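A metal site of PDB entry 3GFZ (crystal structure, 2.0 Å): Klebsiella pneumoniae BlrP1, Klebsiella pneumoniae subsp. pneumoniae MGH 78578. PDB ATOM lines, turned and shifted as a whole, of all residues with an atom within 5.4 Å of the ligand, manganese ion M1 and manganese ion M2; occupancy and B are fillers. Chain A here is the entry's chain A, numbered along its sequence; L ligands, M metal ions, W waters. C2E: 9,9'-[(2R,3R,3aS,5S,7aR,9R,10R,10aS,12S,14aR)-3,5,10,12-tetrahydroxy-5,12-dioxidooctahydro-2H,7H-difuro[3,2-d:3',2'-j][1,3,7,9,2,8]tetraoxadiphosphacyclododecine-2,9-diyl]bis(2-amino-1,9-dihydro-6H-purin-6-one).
N11 of the ligand lies within hydrogen-bond range of O of Asn 247 (3.4 Å). N1 of the ligand sits at hydrogen-bond distance from OE2 of Glu 370, at 2.7 Å. N11 of the ligand sits at hydrogen-bond distance from OD1 of Asp 223 (2.7 Å). The backbone NH of Phe 389 sits at hydrogen-bond distance from an oxygen (O6) of the ligand (2.8 Å). NZ of Lys 227 is in hydrogen-bond range of O61 of the ligand (3.0 Å). The guanidinium group (NH1) of Arg 200 is in salt-bridge range of an oxygen (O11) of the ligand, 3.0 Å away. NE2 of Gln 182 sits at hydrogen-bond distance from N7 of the ligand, 3.2 Å away. The backbone NH (N) of Ile 199 lies within hydrogen-bond range of a nitrogen (N71) of the ligand (3.1 Å).
O of Glu 280 lies within hydrogen-bond range of N of Leu 248, 3.1 Å away. The side-chain amino group (NZ) of Lys 227 lies close to the backbone carbonyl oxygen (O) of Asn 247 (3.2 Å). The backbone NH of Glu 196 is in hydrogen-bond range of the backbone carbonyl oxygen of Gln 182 (2.8 Å). NZ of Lys 227 lies within salt-bridge range of OD1 of Asp 223, 2.8 Å away. The backbone carbonyl oxygen of Val 369 lies within hydrogen-bond range of the backbone NH of Phe 389, 3.4 Å away. The side-chain hydroxyl (OG) of Ser 226 sits at hydrogen-bond distance from the side-chain amino group (NZ) of Lys 227 (3.2 Å). The side-chain amide oxygen (OE1) of Gln 182 is in hydrogen-bond range of the side-chain amide nitrogen (NE2) of Gln 387, 3.0 Å away. N of Gly 368 lies within hydrogen-bond range of O of Gln 387 (2.9 Å).
Phe 179 touches the ligand (CE2 to O61, 3.9 Å). Leu 198 touches the ligand. CD of Pro 207 touches O21 of the ligand, at 3.7 Å. Phe 211 touches the ligand. CG of Leu 249 touches N21 of the ligand (3.6 Å). Gly 368 touches the ligand. O of Val 369 touches O6 of the ligand (3.7 Å). Gly 388 touches the ligand (CA to O6, 3.3 Å). Pro 394 touches the ligand (CG to O2', 3.4 Å). Of the 30 residues printed, 21 come within 4 Å of the ligand.
Four residues have an atom within 4 Å of manganese ion M1: Glu 196, Asn 247, Glu 280 and Asp 310.
The nearest printed residue that does not touch manganese ion M2 is Glu 280 (5.2 Å).
Manganese ion M1 is bound by OE2 of Glu 280 (1.9 Å), O2P of the ligand (2.1 Å), OD2 of Asp 310 (2.1 Å), OD1 of Asn 247 (2.2 Å), OE2 of Glu 196 (2.2 Å) and water W3 (2.3 Å). Manganese ion M1 has six donor atoms within binding distance.
O1P of the ligand is bound to manganese ion M2 (2.0 Å). Manganese ion M2 is bound by OD1 of Asp 311, 2.1 Å away. OE1 of Glu 367 binds manganese ion M2 (2.2 Å). The side-chain carboxylate (OD1) of Asp 310 binds manganese ion M2 (2.4 Å). OE2 of Glu 367 is bound to manganese ion M2 (2.4 Å).
Water W3 lies within hydrogen-bond range of the side-chain carboxylate of Glu 196, the side-chain amino group of Lys 331 and an oxygen (O5') of the ligand. Water W5 bridges an oxygen (O2A) of the ligand (2.6 Å) and the side-chain carboxylate of Asp 311 (3.2 Å). Water W4 lies within hydrogen-bond range of the backbone NH of Gly 368 (2.8 Å), a nitrogen (N7) of the ligand (3.1 Å) and the backbone carbonyl oxygen of Gln 387 (3.2 Å). Water W1 lies within hydrogen-bond range of the backbone carbonyl oxygen (O) of Ala 197 (2.6 Å), the backbone NH (N) of Asn 247 (3.0 Å) and an oxygen (O61) of the ligand (3.1 Å).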
ATOM      1  N   PHE A 179      23.398 -30.023 -35.318  1.00  0.00           N
ATOM      2  CA  PHE A 179      22.297 -29.562 -34.487  1.00  0.00           C
ATOM      3  C   PHE A 179      21.125 -30.489 -34.649  1.00  0.00           C
ATOM      4  O   PHE A 179      20.770 -30.889 -35.766  1.00  0.00           O
ATOM      5  CB  PHE A 179      21.886 -28.132 -34.840  1.00  0.00           C
ATOM      6  CG  PHE A 179      22.838 -27.102 -34.334  1.00  0.00           C
ATOM      7  CD1 PHE A 179      23.916 -26.715 -35.098  1.00  0.00           C
ATOM      8  CD2 PHE A 179      22.679 -26.560 -33.072  1.00  0.00           C
ATOM      9  CE1 PHE A 179      24.813 -25.791 -34.628  1.00  0.00           C
ATOM     10  CE2 PHE A 179      23.563 -25.618 -32.591  1.00  0.00           C
ATOM     11  CZ  PHE A 179      24.640 -25.231 -33.365  1.00  0.00           C
ATOM     12  N   GLN A 182      14.215 -29.837 -32.043  1.00  0.00           N
ATOM     13  CA  GLN A 182      13.029 -30.281 -31.321  1.00  0.00           C
ATOM     14  C   GLN A 182      11.928 -29.226 -31.497  1.00  0.00           C
ATOM     15  O   GLN A 182      12.169 -28.028 -31.318  1.00  0.00           O
ATOM     16  CB  GLN A 182      13.317 -30.491 -29.835  1.00  0.00           C
ATOM     17  CG  GLN A 182      12.119 -31.015 -29.025  1.00  0.00           C
ATOM     18  CD  GLN A 182      12.478 -31.345 -27.578  1.00  0.00           C
ATOM     19  OE1 GLN A 182      13.306 -30.684 -26.957  1.00  0.00           O
ATOM     20  NE2 GLN A 182      11.841 -32.376 -27.042  1.00  0.00           N
ATOM     21  N   GLU A 196      13.644 -25.667 -31.630  1.00  0.00           N
ATOM     22  CA  GLU A 196      14.868 -25.346 -30.901  1.00  0.00           C
ATOM     23  C   GLU A 196      16.045 -26.135 -31.464  1.00  0.00           C
ATOM     24  O   GLU A 196      15.955 -27.340 -31.611  1.00  0.00           O
ATOM     25  CB  GLU A 196      14.750 -25.633 -29.408  1.00  0.00           C
ATOM     26  CG  GLU A 196      16.044 -25.347 -28.674  1.00  0.00           C
ATOM     27  CD  GLU A 196      15.939 -25.395 -27.171  1.00  0.00           C
ATOM     28  OE1 GLU A 196      14.903 -25.848 -26.640  1.00  0.00           O
ATOM     29  OE2 GLU A 196      16.925 -24.935 -26.534  1.00  0.00           O
ATOM     30  N   ALA A 197      17.149 -25.430 -31.731  1.00  0.00           N
ATOM     31  CA  ALA A 197      18.384 -26.038 -32.204  1.00  0.00           C
ATOM     32  C   ALA A 197      19.261 -26.453 -31.008  1.00  0.00           C
ATOM     33  O   ALA A 197      19.668 -25.628 -30.205  1.00  0.00           O
ATOM     34  CB  ALA A 197      19.127 -25.062 -33.083  1.00  0.00           C
ATOM     35  N   LEU A 198      19.561 -27.747 -30.935  1.00  0.00           N
ATOM     36  CA  LEU A 198      20.344 -28.332 -29.846  1.00  0.00           C
ATOM     37  C   LEU A 198      21.656 -28.877 -30.405  1.00  0.00           C
ATOM     38  O   LEU A 198      21.642 -29.772 -31.232  1.00  0.00           O
ATOM     39  CB  LEU A 198      19.547 -29.453 -29.191  1.00  0.00           C
ATOM     40  CG  LEU A 198      18.143 -29.077 -28.729  1.00  0.00           C
ATOM     41  CD1 LEU A 198      17.344 -30.314 -28.328  1.00  0.00           C
ATOM     42  CD2 LEU A 198      18.213 -28.041 -27.596  1.00  0.00           C
ATOM     43  N   ILE A 199      22.789 -28.342 -29.933  1.00  0.00           N
ATOM     44  CA  ILE A 199      24.075 -28.660 -30.557  1.00  0.00           C
ATOM     45  C   ILE A 199      24.484 -30.095 -30.294  1.00  0.00           C
ATOM     46  O   ILE A 199      24.228 -30.648 -29.217  1.00  0.00           O
ATOM     47  CB  ILE A 199      25.199 -27.698 -30.098  1.00  0.00           C
ATOM     48  CG1 ILE A 199      26.386 -27.739 -31.085  1.00  0.00           C
ATOM     49  CG2 ILE A 199      25.657 -28.018 -28.665  1.00  0.00           C
ATOM     50  CD1 ILE A 199      27.327 -26.555 -30.934  1.00  0.00           C
ATOM     51  N   ARG A 200      25.126 -30.694 -31.289  1.00  0.00           N
ATOM     52  CA  ARG A 200      25.595 -32.065 -31.231  1.00  0.00           C
ATOM     53  C   ARG A 200      27.009 -32.135 -31.759  1.00  0.00           C
ATOM     54  O   ARG A 200      27.441 -31.261 -32.509  1.00  0.00           O
ATOM     55  CB  ARG A 200      24.688 -32.949 -32.078  1.00  0.00           C
ATOM     56  CG  ARG A 200      23.261 -33.007 -31.609  1.00  0.00           C
ATOM     57  CD  ARG A 200      23.128 -33.938 -30.437  1.00  0.00           C
ATOM     58  NE  ARG A 200      21.767 -33.980 -29.917  1.00  0.00           N
ATOM     59  CZ  ARG A 200      21.271 -33.178 -28.976  1.00  0.00           C
ATOM     60  NH1 ARG A 200      22.020 -32.260 -28.395  1.00  0.00           N
ATOM     61  NH2 ARG A 200      20.005 -33.329 -28.601  1.00  0.00           N
ATOM     62  N   SER A 206      26.356 -35.581 -27.290  1.00  0.00           N
ATOM     63  CA  SER A 206      25.677 -34.521 -26.529  1.00  0.00           C
ATOM     64  C   SER A 206      26.433 -33.182 -26.578  1.00  0.00           C
ATOM     65  O   SER A 206      27.601 -33.166 -26.971  1.00  0.00           O
ATOM     66  CB  SER A 206      25.545 -34.955 -25.062  1.00  0.00           C
ATOM     67  OG  SER A 206      26.840 -35.014 -24.454  1.00  0.00           O
ATOM     68  N   PRO A 207      25.775 -32.074 -26.177  1.00  0.00           N
ATOM     69  CA  PRO A 207      26.446 -30.767 -26.072  1.00  0.00           C
ATOM     70  C   PRO A 207      27.684 -30.793 -25.176  1.00  0.00           C
ATOM     71  O   PRO A 207      28.691 -30.152 -25.496  1.00  0.00           O
ATOM     72  CB  PRO A 207      25.366 -29.862 -25.460  1.00  0.00           C
ATOM     73  CG  PRO A 207      24.103 -30.473 -25.878  1.00  0.00           C
ATOM     74  CD  PRO A 207      24.348 -31.954 -25.813  1.00  0.00           C
ATOM     75  N   PHE A 211      31.307 -29.676 -26.412  1.00  0.00           N
ATOM     76  CA  PHE A 211      32.127 -28.627 -25.789  1.00  0.00           C
ATOM     77  C   PHE A 211      33.394 -29.128 -25.092  1.00  0.00           C
ATOM     78  O   PHE A 211      34.360 -28.381 -24.970  1.00  0.00           O
ATOM     79  CB  PHE A 211      31.299 -27.764 -24.842  1.00  0.00           C
ATOM     80  CG  PHE A 211      30.470 -26.739 -25.545  1.00  0.00           C
ATOM     81  CD1 PHE A 211      31.063 -25.615 -26.103  1.00  0.00           C
ATOM     82  CD2 PHE A 211      29.101 -26.886 -25.663  1.00  0.00           C
ATOM     83  CE1 PHE A 211      30.317 -24.663 -26.761  1.00  0.00           C
ATOM     84  CE2 PHE A 211      28.345 -25.936 -26.319  1.00  0.00           C
ATOM     85  CZ  PHE A 211      28.952 -24.819 -26.868  1.00  0.00           C
ATOM     86  N   ASP A 223      30.828 -21.498 -29.319  1.00  0.00           N
ATOM     87  CA  ASP A 223      29.389 -21.488 -29.056  1.00  0.00           C
ATOM     88  C   ASP A 223      28.685 -20.541 -30.001  1.00  0.00           C
ATOM     89  O   ASP A 223      27.649 -20.876 -30.592  1.00  0.00           O
ATOM     90  CB  ASP A 223      29.137 -21.058 -27.602  1.00  0.00           C
ATOM     91  CG  ASP A 223      27.670 -21.089 -27.231  1.00  0.00           C
ATOM     92  OD1 ASP A 223      26.929 -21.893 -27.812  1.00  0.00           O
ATOM     93  OD2 ASP A 223      27.249 -20.294 -26.350  1.00  0.00           O
ATOM     94  N   SER A 226      29.278 -21.565 -33.899  1.00  0.00           N
ATOM     95  CA  SER A 226      28.515 -22.751 -34.245  1.00  0.00           C
ATOM     96  C   SER A 226      27.124 -22.433 -34.781  1.00  0.00           C
ATOM     97  O   SER A 226      26.548 -23.228 -35.494  1.00  0.00           O
ATOM     98  CB  SER A 226      28.369 -23.694 -33.040  1.00  0.00           C
ATOM     99  OG  SER A 226      27.530 -23.137 -32.037  1.00  0.00           O
ATOM    100  N   LYS A 227      26.600 -21.258 -34.432  1.00  0.00           N
ATOM    101  CA  LYS A 227      25.238 -20.874 -34.815  1.00  0.00           C
ATOM    102  C   LYS A 227      25.015 -20.692 -36.318  1.00  0.00           C
ATOM    103  O   LYS A 227      23.892 -20.825 -36.791  1.00  0.00           O
ATOM    104  CB  LYS A 227      24.796 -19.638 -34.017  1.00  0.00           C
ATOM    105  CG  LYS A 227      24.780 -19.850 -32.492  1.00  0.00           C
ATOM    106  CD  LYS A 227      24.120 -21.182 -32.121  1.00  0.00           C
ATOM    107  CE  LYS A 227      24.091 -21.410 -30.643  1.00  0.00           C
ATOM    108  NZ  LYS A 227      25.342 -21.971 -30.071  1.00  0.00           N
ATOM    109  N   ASN A 247      20.369 -21.543 -28.380  1.00  0.00           N
ATOM    110  CA  ASN A 247      20.936 -21.414 -27.047  1.00  0.00           C
ATOM    111  C   ASN A 247      22.308 -20.774 -27.120  1.00  0.00           C
ATOM    112  O   ASN A 247      23.138 -21.199 -27.920  1.00  0.00           O
ATOM    113  CB  ASN A 247      21.108 -22.777 -26.386  1.00  0.00           C
ATOM    114  CG  ASN A 247      19.800 -23.466 -26.145  1.00  0.00           C
ATOM    115  OD1 ASN A 247      19.079 -23.123 -25.211  1.00  0.00           O
ATOM    116  ND2 ASN A 247      19.489 -24.467 -26.967  1.00  0.00           N
ATOM    117  N   LEU A 248      22.561 -19.775 -26.280  1.00  0.00           N
ATOM    118  CA  LEU A 248      23.879 -19.130 -26.225  1.00  0.00           C
ATOM    119  C   LEU A 248      24.235 -18.764 -24.793  1.00  0.00           C
ATOM    120  O   LEU A 248      23.366 -18.370 -24.026  1.00  0.00           O
ATOM    121  CB  LEU A 248      23.881 -17.852 -27.085  1.00  0.00           C
ATOM    122  CG  LEU A 248      24.193 -17.953 -28.582  1.00  0.00           C
ATOM    123  CD1 LEU A 248      24.027 -16.579 -29.256  1.00  0.00           C
ATOM    124  CD2 LEU A 248      25.595 -18.474 -28.841  1.00  0.00           C
ATOM    125  N   LEU A 249      25.512 -18.912 -24.448  1.00  0.00           N
ATOM    126  CA  LEU A 249      26.032 -18.407 -23.179  1.00  0.00           C
ATOM    127  C   LEU A 249      26.104 -16.892 -23.287  1.00  0.00           C
ATOM    128  O   LEU A 249      26.570 -16.362 -24.298  1.00  0.00           O
ATOM    129  CB  LEU A 249      27.442 -18.950 -22.911  1.00  0.00           C
ATOM    130  CG  LEU A 249      27.637 -20.460 -22.807  1.00  0.00           C
ATOM    131  CD1 LEU A 249      29.116 -20.809 -22.856  1.00  0.00           C
ATOM    132  CD2 LEU A 249      27.004 -21.013 -21.551  1.00  0.00           C
ATOM    133  N   GLU A 280      17.979 -18.087 -26.650  1.00  0.00           N
ATOM    134  CA  GLU A 280      17.727 -18.626 -25.311  1.00  0.00           C
ATOM    135  C   GLU A 280      18.952 -18.450 -24.419  1.00  0.00           C
ATOM    136  O   GLU A 280      20.022 -18.952 -24.738  1.00  0.00           O
ATOM    137  CB  GLU A 280      17.369 -20.109 -25.352  1.00  0.00           C
ATOM    138  CG  GLU A 280      16.147 -20.415 -26.193  1.00  0.00           C
ATOM    139  CD  GLU A 280      15.501 -21.757 -25.885  1.00  0.00           C
ATOM    140  OE1 GLU A 280      14.423 -22.029 -26.454  1.00  0.00           O
ATOM    141  OE2 GLU A 280      16.068 -22.558 -25.105  1.00  0.00           O
ATOM    142  N   THR A 282      19.911 -18.919 -20.217  1.00  0.00           N
ATOM    143  CA  THR A 282      19.401 -19.488 -18.985  1.00  0.00           C
ATOM    144  C   THR A 282      19.443 -18.440 -17.890  1.00  0.00           C
ATOM    145  O   THR A 282      20.387 -17.658 -17.798  1.00  0.00           O
ATOM    146  CB  THR A 282      20.190 -20.717 -18.504  1.00  0.00           C
ATOM    147  OG1 THR A 282      21.575 -20.384 -18.433  1.00  0.00           O
ATOM    148  CG2 THR A 282      19.988 -21.874 -19.439  1.00  0.00           C
ATOM    149  N   ASP A 310      15.470 -19.330 -20.561  1.00  0.00           N
ATOM    150  CA  ASP A 310      15.400 -20.780 -20.569  1.00  0.00           C
ATOM    151  C   ASP A 310      15.510 -21.255 -19.121  1.00  0.00           C
ATOM    152  O   ASP A 310      16.095 -20.564 -18.288  1.00  0.00           O
ATOM    153  CB  ASP A 310      16.586 -21.293 -21.388  1.00  0.00           C
ATOM    154  CG  ASP A 310      16.398 -22.693 -21.921  1.00  0.00           C
ATOM    155  OD1 ASP A 310      15.318 -23.326 -21.744  1.00  0.00           O
ATOM    156  OD2 ASP A 310      17.359 -23.165 -22.593  1.00  0.00           O
ATOM    157  N   ASP A 311      14.937 -22.419 -18.835  1.00  0.00           N
ATOM    158  CA  ASP A 311      15.020 -23.029 -17.493  1.00  0.00           C
ATOM    159  C   ASP A 311      14.585 -22.073 -16.401  1.00  0.00           C
ATOM    160  O   ASP A 311      15.181 -22.013 -15.329  1.00  0.00           O
ATOM    161  CB  ASP A 311      16.437 -23.549 -17.208  1.00  0.00           C
ATOM    162  CG  ASP A 311      16.923 -24.522 -18.255  1.00  0.00           C
ATOM    163  OD1 ASP A 311      16.074 -25.188 -18.883  1.00  0.00           O
ATOM    164  OD2 ASP A 311      18.147 -24.626 -18.432  1.00  0.00           O
ATOM    165  N   LYS A 331      10.668 -19.989 -20.627  1.00  0.00           N
ATOM    166  CA  LYS A 331      10.522 -21.439 -20.727  1.00  0.00           C
ATOM    167  C   LYS A 331      10.573 -22.001 -19.314  1.00  0.00           C
ATOM    168  O   LYS A 331      11.597 -21.911 -18.663  1.00  0.00           O
ATOM    169  CB  LYS A 331      11.608 -22.019 -21.618  1.00  0.00           C
ATOM    170  CG  LYS A 331      11.683 -21.324 -22.966  1.00  0.00           C
ATOM    171  CD  LYS A 331      12.657 -22.003 -23.916  1.00  0.00           C
ATOM    172  CE  LYS A 331      12.010 -23.181 -24.601  1.00  0.00           C
ATOM    173  NZ  LYS A 331      12.759 -23.634 -25.793  1.00  0.00           N
ATOM    174  N   GLU A 367       8.733 -26.874 -20.517  1.00  0.00           N
ATOM    175  CA  GLU A 367       9.762 -27.801 -20.949  1.00  0.00           C
ATOM    176  C   GLU A 367       9.689 -29.142 -20.238  1.00  0.00           C
ATOM    177  O   GLU A 367       9.226 -29.215 -19.112  1.00  0.00           O
ATOM    178  CB  GLU A 367      11.154 -27.279 -20.621  1.00  0.00           C
ATOM    179  CG  GLU A 367      11.526 -25.945 -21.127  1.00  0.00           C
ATOM    180  CD  GLU A 367      13.018 -25.718 -20.971  1.00  0.00           C
ATOM    181  OE1 GLU A 367      13.783 -26.349 -21.726  1.00  0.00           O
ATOM    182  OE2 GLU A 367      13.436 -24.937 -20.084  1.00  0.00           O
ATOM    183  N   GLY A 368      10.232 -30.165 -20.884  1.00  0.00           N
ATOM    184  CA  GLY A 368      10.400 -31.479 -20.256  1.00  0.00           C
ATOM    185  C   GLY A 368       9.101 -32.241 -20.062  1.00  0.00           C
ATOM    186  O   GLY A 368       8.997 -33.046 -19.146  1.00  0.00           O
ATOM    187  N   VAL A 369       8.140 -32.001 -20.949  1.00  0.00           N
ATOM    188  CA  VAL A 369       6.808 -32.610 -20.833  1.00  0.00           C
ATOM    189  C   VAL A 369       6.864 -34.050 -21.384  1.00  0.00           C
ATOM    190  O   VAL A 369       7.002 -34.256 -22.589  1.00  0.00           O
ATOM    191  CB  VAL A 369       5.732 -31.764 -21.572  1.00  0.00           C
ATOM    192  CG1 VAL A 369       4.346 -32.304 -21.303  1.00  0.00           C
ATOM    193  CG2 VAL A 369       5.775 -30.317 -21.115  1.00  0.00           C
ATOM    194  N   GLU A 370       6.771 -35.018 -20.488  1.00  0.00           N
ATOM    195  CA  GLU A 370       6.989 -36.420 -20.789  1.00  0.00           C
ATOM    196  C   GLU A 370       5.737 -37.283 -20.775  1.00  0.00           C
ATOM    197  O   GLU A 370       5.728 -38.350 -21.377  1.00  0.00           O
ATOM    198  CB  GLU A 370       8.003 -36.990 -19.792  1.00  0.00           C
ATOM    199  CG  GLU A 370       9.347 -36.316 -19.874  1.00  0.00           C
ATOM    200  CD  GLU A 370      10.418 -36.974 -19.038  1.00  0.00           C
ATOM    201  OE1 GLU A 370      10.101 -37.699 -18.061  1.00  0.00           O
ATOM    202  OE2 GLU A 370      11.595 -36.747 -19.347  1.00  0.00           O
ATOM    203  N   GLN A 387       7.144 -28.260 -24.908  1.00  0.00           N
ATOM    204  CA  GLN A 387       8.334 -28.862 -25.467  1.00  0.00           C
ATOM    205  C   GLN A 387       8.628 -30.087 -24.620  1.00  0.00           C
ATOM    206  O   GLN A 387       8.764 -30.006 -23.410  1.00  0.00           O
ATOM    207  CB  GLN A 387       9.488 -27.873 -25.408  1.00  0.00           C
ATOM    208  CG  GLN A 387      10.701 -28.319 -26.225  1.00  0.00           C
ATOM    209  CD  GLN A 387      11.829 -27.345 -26.152  1.00  0.00           C
ATOM    210  OE1 GLN A 387      11.660 -26.210 -25.684  1.00  0.00           O
ATOM    211  NE2 GLN A 387      13.005 -27.761 -26.612  1.00  0.00           N
ATOM    212  N   GLY A 388       8.703 -31.241 -25.266  1.00  0.00           N
ATOM    213  CA  GLY A 388       9.044 -32.431 -24.549  1.00  0.00           C
ATOM    214  C   GLY A 388       8.918 -33.660 -25.407  1.00  0.00           C
ATOM    215  O   GLY A 388       8.306 -33.642 -26.483  1.00  0.00           O
ATOM    216  N   PHE A 389       9.486 -34.740 -24.889  1.00  0.00           N
ATOM    217  CA  PHE A 389       9.482 -36.025 -25.556  1.00  0.00           C
ATOM    218  C   PHE A 389       8.080 -36.584 -25.789  1.00  0.00           C
ATOM    219  O   PHE A 389       7.896 -37.436 -26.649  1.00  0.00           O
ATOM    220  CB  PHE A 389      10.283 -37.029 -24.739  1.00  0.00           C
ATOM    221  CG  PHE A 389      11.761 -36.715 -24.618  1.00  0.00           C
ATOM    222  CD1 PHE A 389      12.403 -35.832 -25.477  1.00  0.00           C
ATOM    223  CD2 PHE A 389      12.506 -37.344 -23.642  1.00  0.00           C
ATOM    224  CE1 PHE A 389      13.763 -35.594 -25.355  1.00  0.00           C
ATOM    225  CE2 PHE A 389      13.865 -37.096 -23.521  1.00  0.00           C
ATOM    226  CZ  PHE A 389      14.480 -36.229 -24.375  1.00  0.00           C
ATOM    227  N   LEU A 390       7.083 -36.125 -25.021  1.00  0.00           N
ATOM    228  CA  LEU A 390       5.709 -36.525 -25.259  1.00  0.00           C
ATOM    229  C   LEU A 390       5.251 -36.195 -26.683  1.00  0.00           C
ATOM    230  O   LEU A 390       4.561 -36.991 -27.322  1.00  0.00           O
ATOM    231  CB  LEU A 390       4.768 -35.867 -24.251  1.00  0.00           C
ATOM    232  CG  LEU A 390       3.297 -36.320 -24.302  1.00  0.00           C
ATOM    233  CD1 LEU A 390       3.160 -37.748 -23.808  1.00  0.00           C
ATOM    234  CD2 LEU A 390       2.436 -35.388 -23.487  1.00  0.00           C
ATOM    235  N   PRO A 394      14.131 -34.664 -30.146  1.00  0.00           N
ATOM    236  CA  PRO A 394      15.108 -34.006 -31.010  1.00  0.00           C
ATOM    237  C   PRO A 394      15.554 -34.911 -32.158  1.00  0.00           C
ATOM    238  O   PRO A 394      15.730 -36.123 -31.974  1.00  0.00           O
ATOM    239  CB  PRO A 394      16.277 -33.727 -30.078  1.00  0.00           C
ATOM    240  CG  PRO A 394      15.671 -33.655 -28.733  1.00  0.00           C
ATOM    241  CD  PRO A 394      14.579 -34.659 -28.737  1.00  0.00           C
HETATM  242  P1  C2E L   1      17.921 -26.819 -22.903  1.00  0.00           P
HETATM  243  O2P C2E L   1      18.169 -25.786 -23.986  1.00  0.00           O
HETATM  244  O1P C2E L   1      17.320 -26.319 -21.622  1.00  0.00           O
HETATM  245  O5' C2E L   1      16.842 -27.912 -23.307  1.00  0.00           O
HETATM  246  C5' C2E L   1      16.974 -28.945 -24.243  1.00  0.00           C
HETATM  247  C4' C2E L   1      17.319 -30.258 -23.527  1.00  0.00           C
HETATM  248  O4' C2E L   1      16.245 -30.926 -22.852  1.00  0.00           O
HETATM  249  C3' C2E L   1      17.725 -31.220 -24.615  1.00  0.00           C
HETATM  250  O3' C2E L   1      18.796 -31.979 -24.145  1.00  0.00           O
HETATM  251  C2' C2E L   1      16.585 -32.139 -24.762  1.00  0.00           C
HETATM  252  O2' C2E L   1      16.807 -33.196 -25.536  1.00  0.00           O
HETATM  253  C1' C2E L   1      15.931 -32.158 -23.595  1.00  0.00           C
HETATM  254  N9  C2E L   1      14.616 -32.530 -23.520  1.00  0.00           N
HETATM  255  C8  C2E L   1      13.710 -32.016 -24.275  1.00  0.00           C
HETATM  256  N7  C2E L   1      12.568 -32.542 -23.937  1.00  0.00           N
HETATM  257  C5  C2E L   1      12.741 -33.405 -22.910  1.00  0.00           C
HETATM  258  C6  C2E L   1      11.883 -34.228 -22.170  1.00  0.00           C
HETATM  259  O6  C2E L   1      10.654 -34.268 -22.385  1.00  0.00           O
HETATM  260  N1  C2E L   1      12.415 -34.975 -21.198  1.00  0.00           N
HETATM  261  C2  C2E L   1      13.738 -34.953 -20.933  1.00  0.00           C
HETATM  262  N2  C2E L   1      14.181 -35.749 -19.936  1.00  0.00           N
HETATM  263  N3  C2E L   1      14.601 -34.178 -21.630  1.00  0.00           N
HETATM  264  C4  C2E L   1      14.099 -33.395 -22.628  1.00  0.00           C
HETATM  265  P11 C2E L   1      20.221 -31.640 -24.717  1.00  0.00           P
HETATM  266  O21 C2E L   1      21.096 -32.955 -24.482  1.00  0.00           O
HETATM  267  O11 C2E L   1      20.092 -31.461 -26.292  1.00  0.00           O
HETATM  268  O5A C2E L   1      20.710 -30.188 -24.236  1.00  0.00           O
HETATM  269  C5A C2E L   1      21.348 -30.047 -22.963  1.00  0.00           C
HETATM  270  C4A C2E L   1      21.482 -28.527 -22.847  1.00  0.00           C
HETATM  271  O4A C2E L   1      22.684 -28.085 -23.459  1.00  0.00           O
HETATM  272  C3A C2E L   1      20.395 -27.613 -23.418  1.00  0.00           C
HETATM  273  O3A C2E L   1      19.310 -27.524 -22.508  1.00  0.00           O
HETATM  274  C2A C2E L   1      21.163 -26.342 -23.625  1.00  0.00           C
HETATM  275  O2A C2E L   1      21.460 -25.766 -22.444  1.00  0.00           O
HETATM  276  C1A C2E L   1      22.255 -26.901 -24.155  1.00  0.00           C
HETATM  277  N91 C2E L   1      22.710 -26.508 -25.376  1.00  0.00           N
HETATM  278  C81 C2E L   1      22.216 -27.110 -26.459  1.00  0.00           C
HETATM  279  N71 C2E L   1      22.799 -26.475 -27.513  1.00  0.00           N
HETATM  280  C51 C2E L   1      23.623 -25.505 -27.047  1.00  0.00           C
HETATM  281  C61 C2E L   1      24.434 -24.584 -27.677  1.00  0.00           C
HETATM  282  O61 C2E L   1      24.497 -24.553 -28.921  1.00  0.00           O
HETATM  283  N11 C2E L   1      25.156 -23.714 -26.917  1.00  0.00           N
HETATM  284  C21 C2E L   1      25.069 -23.745 -25.559  1.00  0.00           C
HETATM  285  N21 C2E L   1      25.781 -22.877 -24.798  1.00  0.00           N
HETATM  286  N31 C2E L   1      24.272 -24.632 -24.923  1.00  0.00           N
HETATM  287  C41 C2E L   1      23.546 -25.512 -25.651  1.00  0.00           C
HETATM  288 MN    MN M   1      17.169 -24.021 -24.513  1.00  0.00          MN
HETATM  289 MN    MN M   2      15.618 -25.533 -20.911  1.00  0.00          MN
HETATM  290  O   HOH W   1      21.607 -23.909 -29.798  1.00  0.00           O
HETATM  291  O   HOH W   2      18.321 -34.980 -24.547  1.00  0.00           O
HETATM  292  O   HOH W   3      15.166 -24.970 -23.820  1.00  0.00           O
HETATM  293  O   HOH W   4      11.932 -29.674 -23.060  1.00  0.00           O
HETATM  294  O   HOH W   5      19.491 -24.402 -21.320  1.00  0.00           O
